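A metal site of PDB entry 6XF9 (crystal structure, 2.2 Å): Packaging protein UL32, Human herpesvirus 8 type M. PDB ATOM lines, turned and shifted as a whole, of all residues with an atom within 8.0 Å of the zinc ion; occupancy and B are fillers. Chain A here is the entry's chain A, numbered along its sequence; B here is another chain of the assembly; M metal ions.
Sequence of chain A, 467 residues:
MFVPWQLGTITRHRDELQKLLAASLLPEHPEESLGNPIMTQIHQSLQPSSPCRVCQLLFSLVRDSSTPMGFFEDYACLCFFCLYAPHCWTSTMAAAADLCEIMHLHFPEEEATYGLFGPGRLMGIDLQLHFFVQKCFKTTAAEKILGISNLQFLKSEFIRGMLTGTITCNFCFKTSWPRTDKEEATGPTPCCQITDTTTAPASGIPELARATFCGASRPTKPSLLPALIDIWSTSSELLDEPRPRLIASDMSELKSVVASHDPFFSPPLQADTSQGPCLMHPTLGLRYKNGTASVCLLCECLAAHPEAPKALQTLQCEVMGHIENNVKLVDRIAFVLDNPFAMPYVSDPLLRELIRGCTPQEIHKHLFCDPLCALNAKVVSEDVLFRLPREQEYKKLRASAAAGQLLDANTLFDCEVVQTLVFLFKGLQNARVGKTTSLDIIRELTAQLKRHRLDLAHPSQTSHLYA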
ATOM      1  N   PRO A  51      -2.055 -15.173 -16.309  1.00  0.00           N
ATOM      2  CA  PRO A  51      -1.445 -15.968 -17.377  1.00  0.00           C
ATOM      3  C   PRO A  51      -0.286 -15.191 -17.976  1.00  0.00           C
ATOM      4  O   PRO A  51      -0.146 -13.982 -17.776  1.00  0.00           O
ATOM      5  CB  PRO A  51      -2.577 -16.166 -18.381  1.00  0.00           C
ATOM      6  CG  PRO A  51      -3.501 -15.016 -18.123  1.00  0.00           C
ATOM      7  CD  PRO A  51      -3.439 -14.809 -16.638  1.00  0.00           C
ATOM      8  N   CYS A  52       0.580 -15.935 -18.668  1.00  0.00           N
ATOM      9  CA  CYS A  52       1.597 -15.303 -19.500  1.00  0.00           C
ATOM     10  C   CYS A  52       0.952 -14.974 -20.834  1.00  0.00           C
ATOM     11  O   CYS A  52       0.479 -15.864 -21.531  1.00  0.00           O
ATOM     12  CB  CYS A  52       2.788 -16.237 -19.681  1.00  0.00           C
ATOM     13  SG  CYS A  52       4.003 -15.501 -20.748  1.00  0.00           S
ATOM     14  N   ARG A  53       0.868 -13.699 -21.177  1.00  0.00           N
ATOM     15  CA  ARG A  53       0.148 -13.378 -22.405  1.00  0.00           C
ATOM     16  C   ARG A  53       0.820 -13.999 -23.622  1.00  0.00           C
ATOM     17  O   ARG A  53       0.134 -14.494 -24.529  1.00  0.00           O
ATOM     18  CB  ARG A  53      -0.004 -11.863 -22.547  1.00  0.00           C
ATOM     19  CG  ARG A  53      -0.962 -11.295 -21.525  1.00  0.00           C
ATOM     20  CD  ARG A  53      -1.054  -9.824 -21.641  1.00  0.00           C
ATOM     21  NE  ARG A  53      -2.130  -9.463 -22.558  1.00  0.00           N
ATOM     22  CZ  ARG A  53      -3.407  -9.403 -22.201  1.00  0.00           C
ATOM     23  NH1 ARG A  53      -3.750  -9.694 -20.948  1.00  0.00           N
ATOM     24  NH2 ARG A  53      -4.333  -9.071 -23.088  1.00  0.00           N
ATOM     25  N   VAL A  54       2.155 -14.054 -23.639  1.00  0.00           N
ATOM     26  CA  VAL A  54       2.842 -14.641 -24.792  1.00  0.00           C
ATOM     27  C   VAL A  54       2.621 -16.137 -24.851  1.00  0.00           C
ATOM     28  O   VAL A  54       2.387 -16.705 -25.927  1.00  0.00           O
ATOM     29  CB  VAL A  54       4.339 -14.294 -24.770  1.00  0.00           C
ATOM     30  CG1 VAL A  54       5.029 -15.017 -25.878  1.00  0.00           C
ATOM     31  CG2 VAL A  54       4.539 -12.806 -24.938  1.00  0.00           C
ATOM     32  N   CYS A  55       2.688 -16.832 -23.710  1.00  0.00           N
ATOM     33  CA  CYS A  55       2.318 -18.240 -23.714  1.00  0.00           C
ATOM     34  C   CYS A  55       0.887 -18.438 -24.181  1.00  0.00           C
ATOM     35  O   CYS A  55       0.581 -19.457 -24.802  1.00  0.00           O
ATOM     36  CB  CYS A  55       2.461 -18.850 -22.327  1.00  0.00           C
ATOM     37  SG  CYS A  55       4.111 -19.225 -21.800  1.00  0.00           S
ATOM     38  N   GLN A  56      -0.016 -17.497 -23.856  1.00  0.00           N
ATOM     39  CA  GLN A  56      -1.420 -17.628 -24.251  1.00  0.00           C
ATOM     40  C   GLN A  56      -1.607 -17.368 -25.742  1.00  0.00           C
ATOM     41  O   GLN A  56      -2.430 -18.008 -26.397  1.00  0.00           O
ATOM     42  CB  GLN A  56      -2.296 -16.698 -23.408  1.00  0.00           C
ATOM     43  CG  GLN A  56      -2.383 -17.168 -21.952  1.00  0.00           C
ATOM     44  CD  GLN A  56      -3.191 -18.455 -21.784  1.00  0.00           C
ATOM     45  OE1 GLN A  56      -3.795 -18.951 -22.734  1.00  0.00           O
ATOM     46  NE2 GLN A  56      -3.165 -19.033 -20.586  1.00  0.00           N
ATOM     47  N   LEU A  57      -0.852 -16.416 -26.287  1.00  0.00           N
ATOM     48  CA  LEU A  57      -0.868 -16.207 -27.726  1.00  0.00           C
ATOM     49  C   LEU A  57      -0.453 -17.489 -28.459  1.00  0.00           C
ATOM     50  O   LEU A  57      -1.184 -17.981 -29.324  1.00  0.00           O
ATOM     51  CB  LEU A  57       0.064 -15.058 -28.093  1.00  0.00           C
ATOM     52  CG  LEU A  57       0.045 -14.567 -29.517  1.00  0.00           C
ATOM     53  CD1 LEU A  57      -1.351 -14.137 -29.835  1.00  0.00           C
ATOM     54  CD2 LEU A  57       0.955 -13.380 -29.629  1.00  0.00           C
ATOM     55  N   LEU A  58       0.685 -18.072 -28.056  1.00  0.00           N
ATOM     56  CA  LEU A  58       1.242 -19.215 -28.779  1.00  0.00           C
ATOM     57  C   LEU A  58       0.298 -20.411 -28.760  1.00  0.00           C
ATOM     58  O   LEU A  58      -0.027 -20.971 -29.815  1.00  0.00           O
ATOM     59  CB  LEU A  58       2.608 -19.587 -28.225  1.00  0.00           C
ATOM     60  CG  LEU A  58       3.644 -18.468 -28.405  1.00  0.00           C
ATOM     61  CD1 LEU A  58       5.005 -18.809 -27.762  1.00  0.00           C
ATOM     62  CD2 LEU A  58       3.791 -18.114 -29.870  1.00  0.00           C
ATOM     63  N   TYR A  75      10.641 -20.006 -33.930  1.00  0.00           N
ATOM     64  CA  TYR A  75      10.423 -19.605 -32.546  1.00  0.00           C
ATOM     65  C   TYR A  75      11.578 -20.043 -31.658  1.00  0.00           C
ATOM     66  O   TYR A  75      12.050 -19.256 -30.836  1.00  0.00           O
ATOM     67  CB  TYR A  75       9.109 -20.183 -32.016  1.00  0.00           C
ATOM     68  CG  TYR A  75       8.855 -19.960 -30.509  1.00  0.00           C
ATOM     69  CD1 TYR A  75       8.681 -18.682 -29.960  1.00  0.00           C
ATOM     70  CD2 TYR A  75       8.766 -21.044 -29.644  1.00  0.00           C
ATOM     71  CE1 TYR A  75       8.430 -18.514 -28.590  1.00  0.00           C
ATOM     72  CE2 TYR A  75       8.525 -20.881 -28.293  1.00  0.00           C
ATOM     73  CZ  TYR A  75       8.350 -19.627 -27.760  1.00  0.00           C
ATOM     74  OH  TYR A  75       8.106 -19.541 -26.395  1.00  0.00           O
ATOM     75  N   ASP A 126       5.057  -7.993 -20.961  1.00  0.00           N
ATOM     76  CA  ASP A 126       4.726  -9.374 -21.317  1.00  0.00           C
ATOM     77  C   ASP A 126       5.879 -10.031 -22.079  1.00  0.00           C
ATOM     78  O   ASP A 126       6.177 -11.207 -21.874  1.00  0.00           O
ATOM     79  CB  ASP A 126       3.428  -9.377 -22.121  1.00  0.00           C
ATOM     80  CG  ASP A 126       2.281  -8.716 -21.346  1.00  0.00           C
ATOM     81  OD1 ASP A 126       1.954  -9.226 -20.261  1.00  0.00           O
ATOM     82  OD2 ASP A 126       1.734  -7.677 -21.786  1.00  0.00           O
ATOM     83  N   LEU A 127       6.533  -9.266 -22.949  1.00  0.00           N
ATOM     84  CA  LEU A 127       7.760  -9.737 -23.582  1.00  0.00           C
ATOM     85  C   LEU A 127       8.868  -9.929 -22.559  1.00  0.00           C
ATOM     86  O   LEU A 127       9.510 -10.985 -22.530  1.00  0.00           O
ATOM     87  CB  LEU A 127       8.198  -8.751 -24.667  1.00  0.00           C
ATOM     88  CG  LEU A 127       7.130  -8.689 -25.750  1.00  0.00           C
ATOM     89  CD1 LEU A 127       7.366  -7.568 -26.730  1.00  0.00           C
ATOM     90  CD2 LEU A 127       7.071 -10.045 -26.454  1.00  0.00           C
ATOM     91  N   LEU A 129       8.745 -10.545 -19.380  1.00  0.00           N
ATOM     92  CA  LEU A 129       8.506 -11.701 -18.524  1.00  0.00           C
ATOM     93  C   LEU A 129       8.755 -12.992 -19.278  1.00  0.00           C
ATOM     94  O   LEU A 129       9.404 -13.910 -18.757  1.00  0.00           O
ATOM     95  CB  LEU A 129       7.086 -11.688 -17.980  1.00  0.00           C
ATOM     96  CG  LEU A 129       6.801 -10.671 -16.862  1.00  0.00           C
ATOM     97  CD1 LEU A 129       5.342 -10.743 -16.492  1.00  0.00           C
ATOM     98  CD2 LEU A 129       7.661 -10.901 -15.665  1.00  0.00           C
ATOM     99  N   HIS A 130       8.271 -13.081 -20.524  1.00  0.00           N
ATOM    100  CA  HIS A 130       8.298 -14.361 -21.224  1.00  0.00           C
ATOM    101  C   HIS A 130       9.723 -14.695 -21.655  1.00  0.00           C
ATOM    102  O   HIS A 130      10.223 -15.788 -21.395  1.00  0.00           O
ATOM    103  CB  HIS A 130       7.343 -14.324 -22.421  1.00  0.00           C
ATOM    104  CG  HIS A 130       7.270 -15.602 -23.197  1.00  0.00           C
ATOM    105  ND1 HIS A 130       6.492 -16.677 -22.799  1.00  0.00           N
ATOM    106  CD2 HIS A 130       7.844 -15.987 -24.366  1.00  0.00           C
ATOM    107  CE1 HIS A 130       6.622 -17.668 -23.665  1.00  0.00           C
ATOM    108  NE2 HIS A 130       7.434 -17.267 -24.636  1.00  0.00           N
ATOM    109  N   PHE A 131      10.413 -13.740 -22.236  1.00  0.00           N
ATOM    110  CA  PHE A 131      11.681 -14.058 -22.858  1.00  0.00           C
ATOM    111  C   PHE A 131      12.869 -13.842 -21.931  1.00  0.00           C
ATOM    112  O   PHE A 131      13.953 -14.380 -22.203  1.00  0.00           O
ATOM    113  CB  PHE A 131      11.845 -13.239 -24.159  1.00  0.00           C
ATOM    114  CG  PHE A 131      10.909 -13.698 -25.287  1.00  0.00           C
ATOM    115  CD1 PHE A 131      11.083 -14.925 -25.898  1.00  0.00           C
ATOM    116  CD2 PHE A 131       9.891 -12.878 -25.738  1.00  0.00           C
ATOM    117  CE1 PHE A 131      10.226 -15.355 -26.917  1.00  0.00           C
ATOM    118  CE2 PHE A 131       9.038 -13.292 -26.763  1.00  0.00           C
ATOM    119  CZ  PHE A 131       9.206 -14.537 -27.358  1.00  0.00           C
ATOM    120  N   GLN A 134      11.159 -14.642 -16.716  1.00  0.00           N
ATOM    121  CA  GLN A 134      10.785 -15.992 -16.320  1.00  0.00           C
ATOM    122  C   GLN A 134      11.345 -17.063 -17.247  1.00  0.00           C
ATOM    123  O   GLN A 134      11.498 -18.217 -16.810  1.00  0.00           O
ATOM    124  CB  GLN A 134       9.265 -16.149 -16.265  1.00  0.00           C
ATOM    125  CG  GLN A 134       8.469 -14.978 -15.678  1.00  0.00           C
ATOM    126  CD  GLN A 134       8.624 -14.779 -14.183  1.00  0.00           C
ATOM    127  OE1 GLN A 134       9.667 -15.115 -13.594  1.00  0.00           O
ATOM    128  NE2 GLN A 134       7.569 -14.244 -13.549  1.00  0.00           N
ATOM    129  N   LYS A 135      11.677 -16.694 -18.486  1.00  0.00           N
ATOM    130  CA  LYS A 135      12.191 -17.635 -19.503  1.00  0.00           C
ATOM    131  C   LYS A 135      11.253 -18.830 -19.734  1.00  0.00           C
ATOM    132  O   LYS A 135      11.636 -19.971 -19.481  1.00  0.00           O
ATOM    133  CB  LYS A 135      13.580 -18.134 -19.106  1.00  0.00           C
ATOM    134  CG  LYS A 135      14.635 -17.033 -19.034  1.00  0.00           C
ATOM    135  CD  LYS A 135      15.995 -17.601 -18.669  1.00  0.00           C
ATOM    136  CE  LYS A 135      17.068 -16.511 -18.657  1.00  0.00           C
ATOM    137  NZ  LYS A 135      16.748 -15.440 -17.683  1.00  0.00           N
ATOM    138  N   CYS A 136      10.033 -18.565 -20.202  1.00  0.00           N
ATOM    139  CA  CYS A 136       9.032 -19.637 -20.297  1.00  0.00           C
ATOM    140  C   CYS A 136       9.432 -20.763 -21.243  1.00  0.00           C
ATOM    141  O   CYS A 136       8.880 -21.861 -21.153  1.00  0.00           O
ATOM    142  CB  CYS A 136       7.687 -19.093 -20.758  1.00  0.00           C
ATOM    143  SG  CYS A 136       6.976 -17.748 -19.810  1.00  0.00           S
ATOM    144  N   PHE A 137      10.379 -20.514 -22.150  1.00  0.00           N
ATOM    145  CA  PHE A 137      10.758 -21.439 -23.216  1.00  0.00           C
ATOM    146  C   PHE A 137      11.749 -22.502 -22.780  1.00  0.00           C
ATOM    147  O   PHE A 137      11.977 -23.462 -23.523  1.00  0.00           O
ATOM    148  CB  PHE A 137      11.350 -20.672 -24.395  1.00  0.00           C
ATOM    149  CG  PHE A 137      12.476 -19.753 -24.007  1.00  0.00           C
ATOM    150  CD1 PHE A 137      13.751 -20.244 -23.762  1.00  0.00           C
ATOM    151  CD2 PHE A 137      12.246 -18.377 -23.892  1.00  0.00           C
ATOM    152  CE1 PHE A 137      14.799 -19.368 -23.392  1.00  0.00           C
ATOM    153  CE2 PHE A 137      13.271 -17.507 -23.519  1.00  0.00           C
ATOM    154  CZ  PHE A 137      14.546 -17.997 -23.273  1.00  0.00           C
ATOM    155  N   ASN B 326       9.139 -24.403 -19.426  1.00  0.00           N
ATOM    156  CA  ASN B 326       8.985 -23.628 -18.200  1.00  0.00           C
ATOM    157  C   ASN B 326       7.687 -22.841 -18.201  1.00  0.00           C
ATOM    158  O   ASN B 326       7.647 -21.710 -17.724  1.00  0.00           O
ATOM    159  CB  ASN B 326      10.178 -22.689 -18.055  1.00  0.00           C
ATOM    160  CG  ASN B 326      10.400 -22.252 -16.642  1.00  0.00           C
ATOM    161  OD1 ASN B 326       9.928 -22.900 -15.693  1.00  0.00           O
ATOM    162  ND2 ASN B 326      11.095 -21.133 -16.474  1.00  0.00           N
ATOM    163  N   VAL B 327       6.594 -23.410 -18.686  1.00  0.00           N
ATOM    164  CA  VAL B 327       5.291 -22.765 -18.612  1.00  0.00           C
ATOM    165  C   VAL B 327       4.726 -22.939 -17.200  1.00  0.00           C
ATOM    166  O   VAL B 327       4.724 -24.060 -16.656  1.00  0.00           O
ATOM    167  CB  VAL B 327       4.373 -23.349 -19.688  1.00  0.00           C
ATOM    168  CG1 VAL B 327       2.997 -22.770 -19.603  1.00  0.00           C
ATOM    169  CG2 VAL B 327       4.962 -23.012 -21.029  1.00  0.00           C
ATOM    170  N   LYS B 328       4.201 -21.856 -16.618  1.00  0.00           N
ATOM    171  CA  LYS B 328       3.739 -21.818 -15.231  1.00  0.00           C
ATOM    172  C   LYS B 328       2.456 -22.623 -15.024  1.00  0.00           C
ATOM    173  O   LYS B 328       1.640 -22.791 -15.936  1.00  0.00           O
ATOM    174  CB  LYS B 328       3.516 -20.361 -14.783  1.00  0.00           C
ATOM    175  CG  LYS B 328       2.293 -19.684 -15.407  1.00  0.00           C
ATOM    176  CD  LYS B 328       2.368 -18.147 -15.343  1.00  0.00           C
ATOM    177  CE  LYS B 328       1.975 -17.599 -13.980  1.00  0.00           C
ATOM    178  NZ  LYS B 328       2.158 -16.108 -13.878  1.00  0.00           N
ATOM    179  N   ASP B 331      -0.904 -21.521 -16.439  1.00  0.00           N
ATOM    180  CA  ASP B 331      -0.948 -21.678 -17.898  1.00  0.00           C
ATOM    181  C   ASP B 331      -0.956 -23.144 -18.298  1.00  0.00           C
ATOM    182  O   ASP B 331      -1.646 -23.516 -19.255  1.00  0.00           O
ATOM    183  CB  ASP B 331       0.232 -20.958 -18.546  1.00  0.00           C
ATOM    184  CG  ASP B 331       0.056 -19.465 -18.551  1.00  0.00           C
ATOM    185  OD1 ASP B 331      -1.120 -19.068 -18.646  1.00  0.00           O
ATOM    186  OD2 ASP B 331       1.063 -18.711 -18.416  1.00  0.00           O
ATOM    187  N   PHE B 335      -3.802 -24.745 -20.572  1.00  0.00           N
ATOM    188  CA  PHE B 335      -3.486 -25.453 -21.807  1.00  0.00           C
ATOM    189  C   PHE B 335      -4.110 -26.835 -21.803  1.00  0.00           C
ATOM    190  O   PHE B 335      -4.707 -27.262 -22.801  1.00  0.00           O
ATOM    191  CB  PHE B 335      -1.971 -25.604 -22.011  1.00  0.00           C
ATOM    192  CG  PHE B 335      -1.229 -24.322 -22.364  1.00  0.00           C
ATOM    193  CD1 PHE B 335      -1.878 -23.096 -22.454  1.00  0.00           C
ATOM    194  CD2 PHE B 335       0.145 -24.352 -22.629  1.00  0.00           C
ATOM    195  CE1 PHE B 335      -1.165 -21.947 -22.789  1.00  0.00           C
ATOM    196  CE2 PHE B 335       0.850 -23.208 -22.967  1.00  0.00           C
ATOM    197  CZ  PHE B 335       0.201 -22.007 -23.041  1.00  0.00           C
HETATM  198 ZN    ZN M   1       5.266 -17.323 -21.306  1.00  0.00          ZN
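Within 4 Å of the zinc ion: Cys 52, Cys 55, His 130 and Cys 136.
The nearest printed residue that does not touch the zinc ion is Val 54 (4.6 Å).
NE2 of His 130 lies within hydrogen-bond range of OH of Tyr 75 (3.0 Å).
O of His 130 lies close to N of Lys 135 (3.4 Å).
The side-chain sulfur (SG) of Cys 52 lies close to the backbone NH (N) of Val 54.
The backbone NH of Cys 52 sits at hydrogen-bond distance from the side-chain carboxylate of Asp 331 of chain B (2.8 Å).
O of Cys 136 is in hydrogen-bond range of N of Asn 326 of chain B (3.1 Å).
A ring nitrogen (ND1) of His 130 binds the zinc ion (2.0 Å).
The side-chain sulfur (SG) of Cys 55 binds the zinc ion (2.3 Å).
The side-chain sulfur (SG) of Cys 52 is bound to the zinc ion (2.3 Å).
The zinc ion is bound by SG of Cys 136 (2.3 Å).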
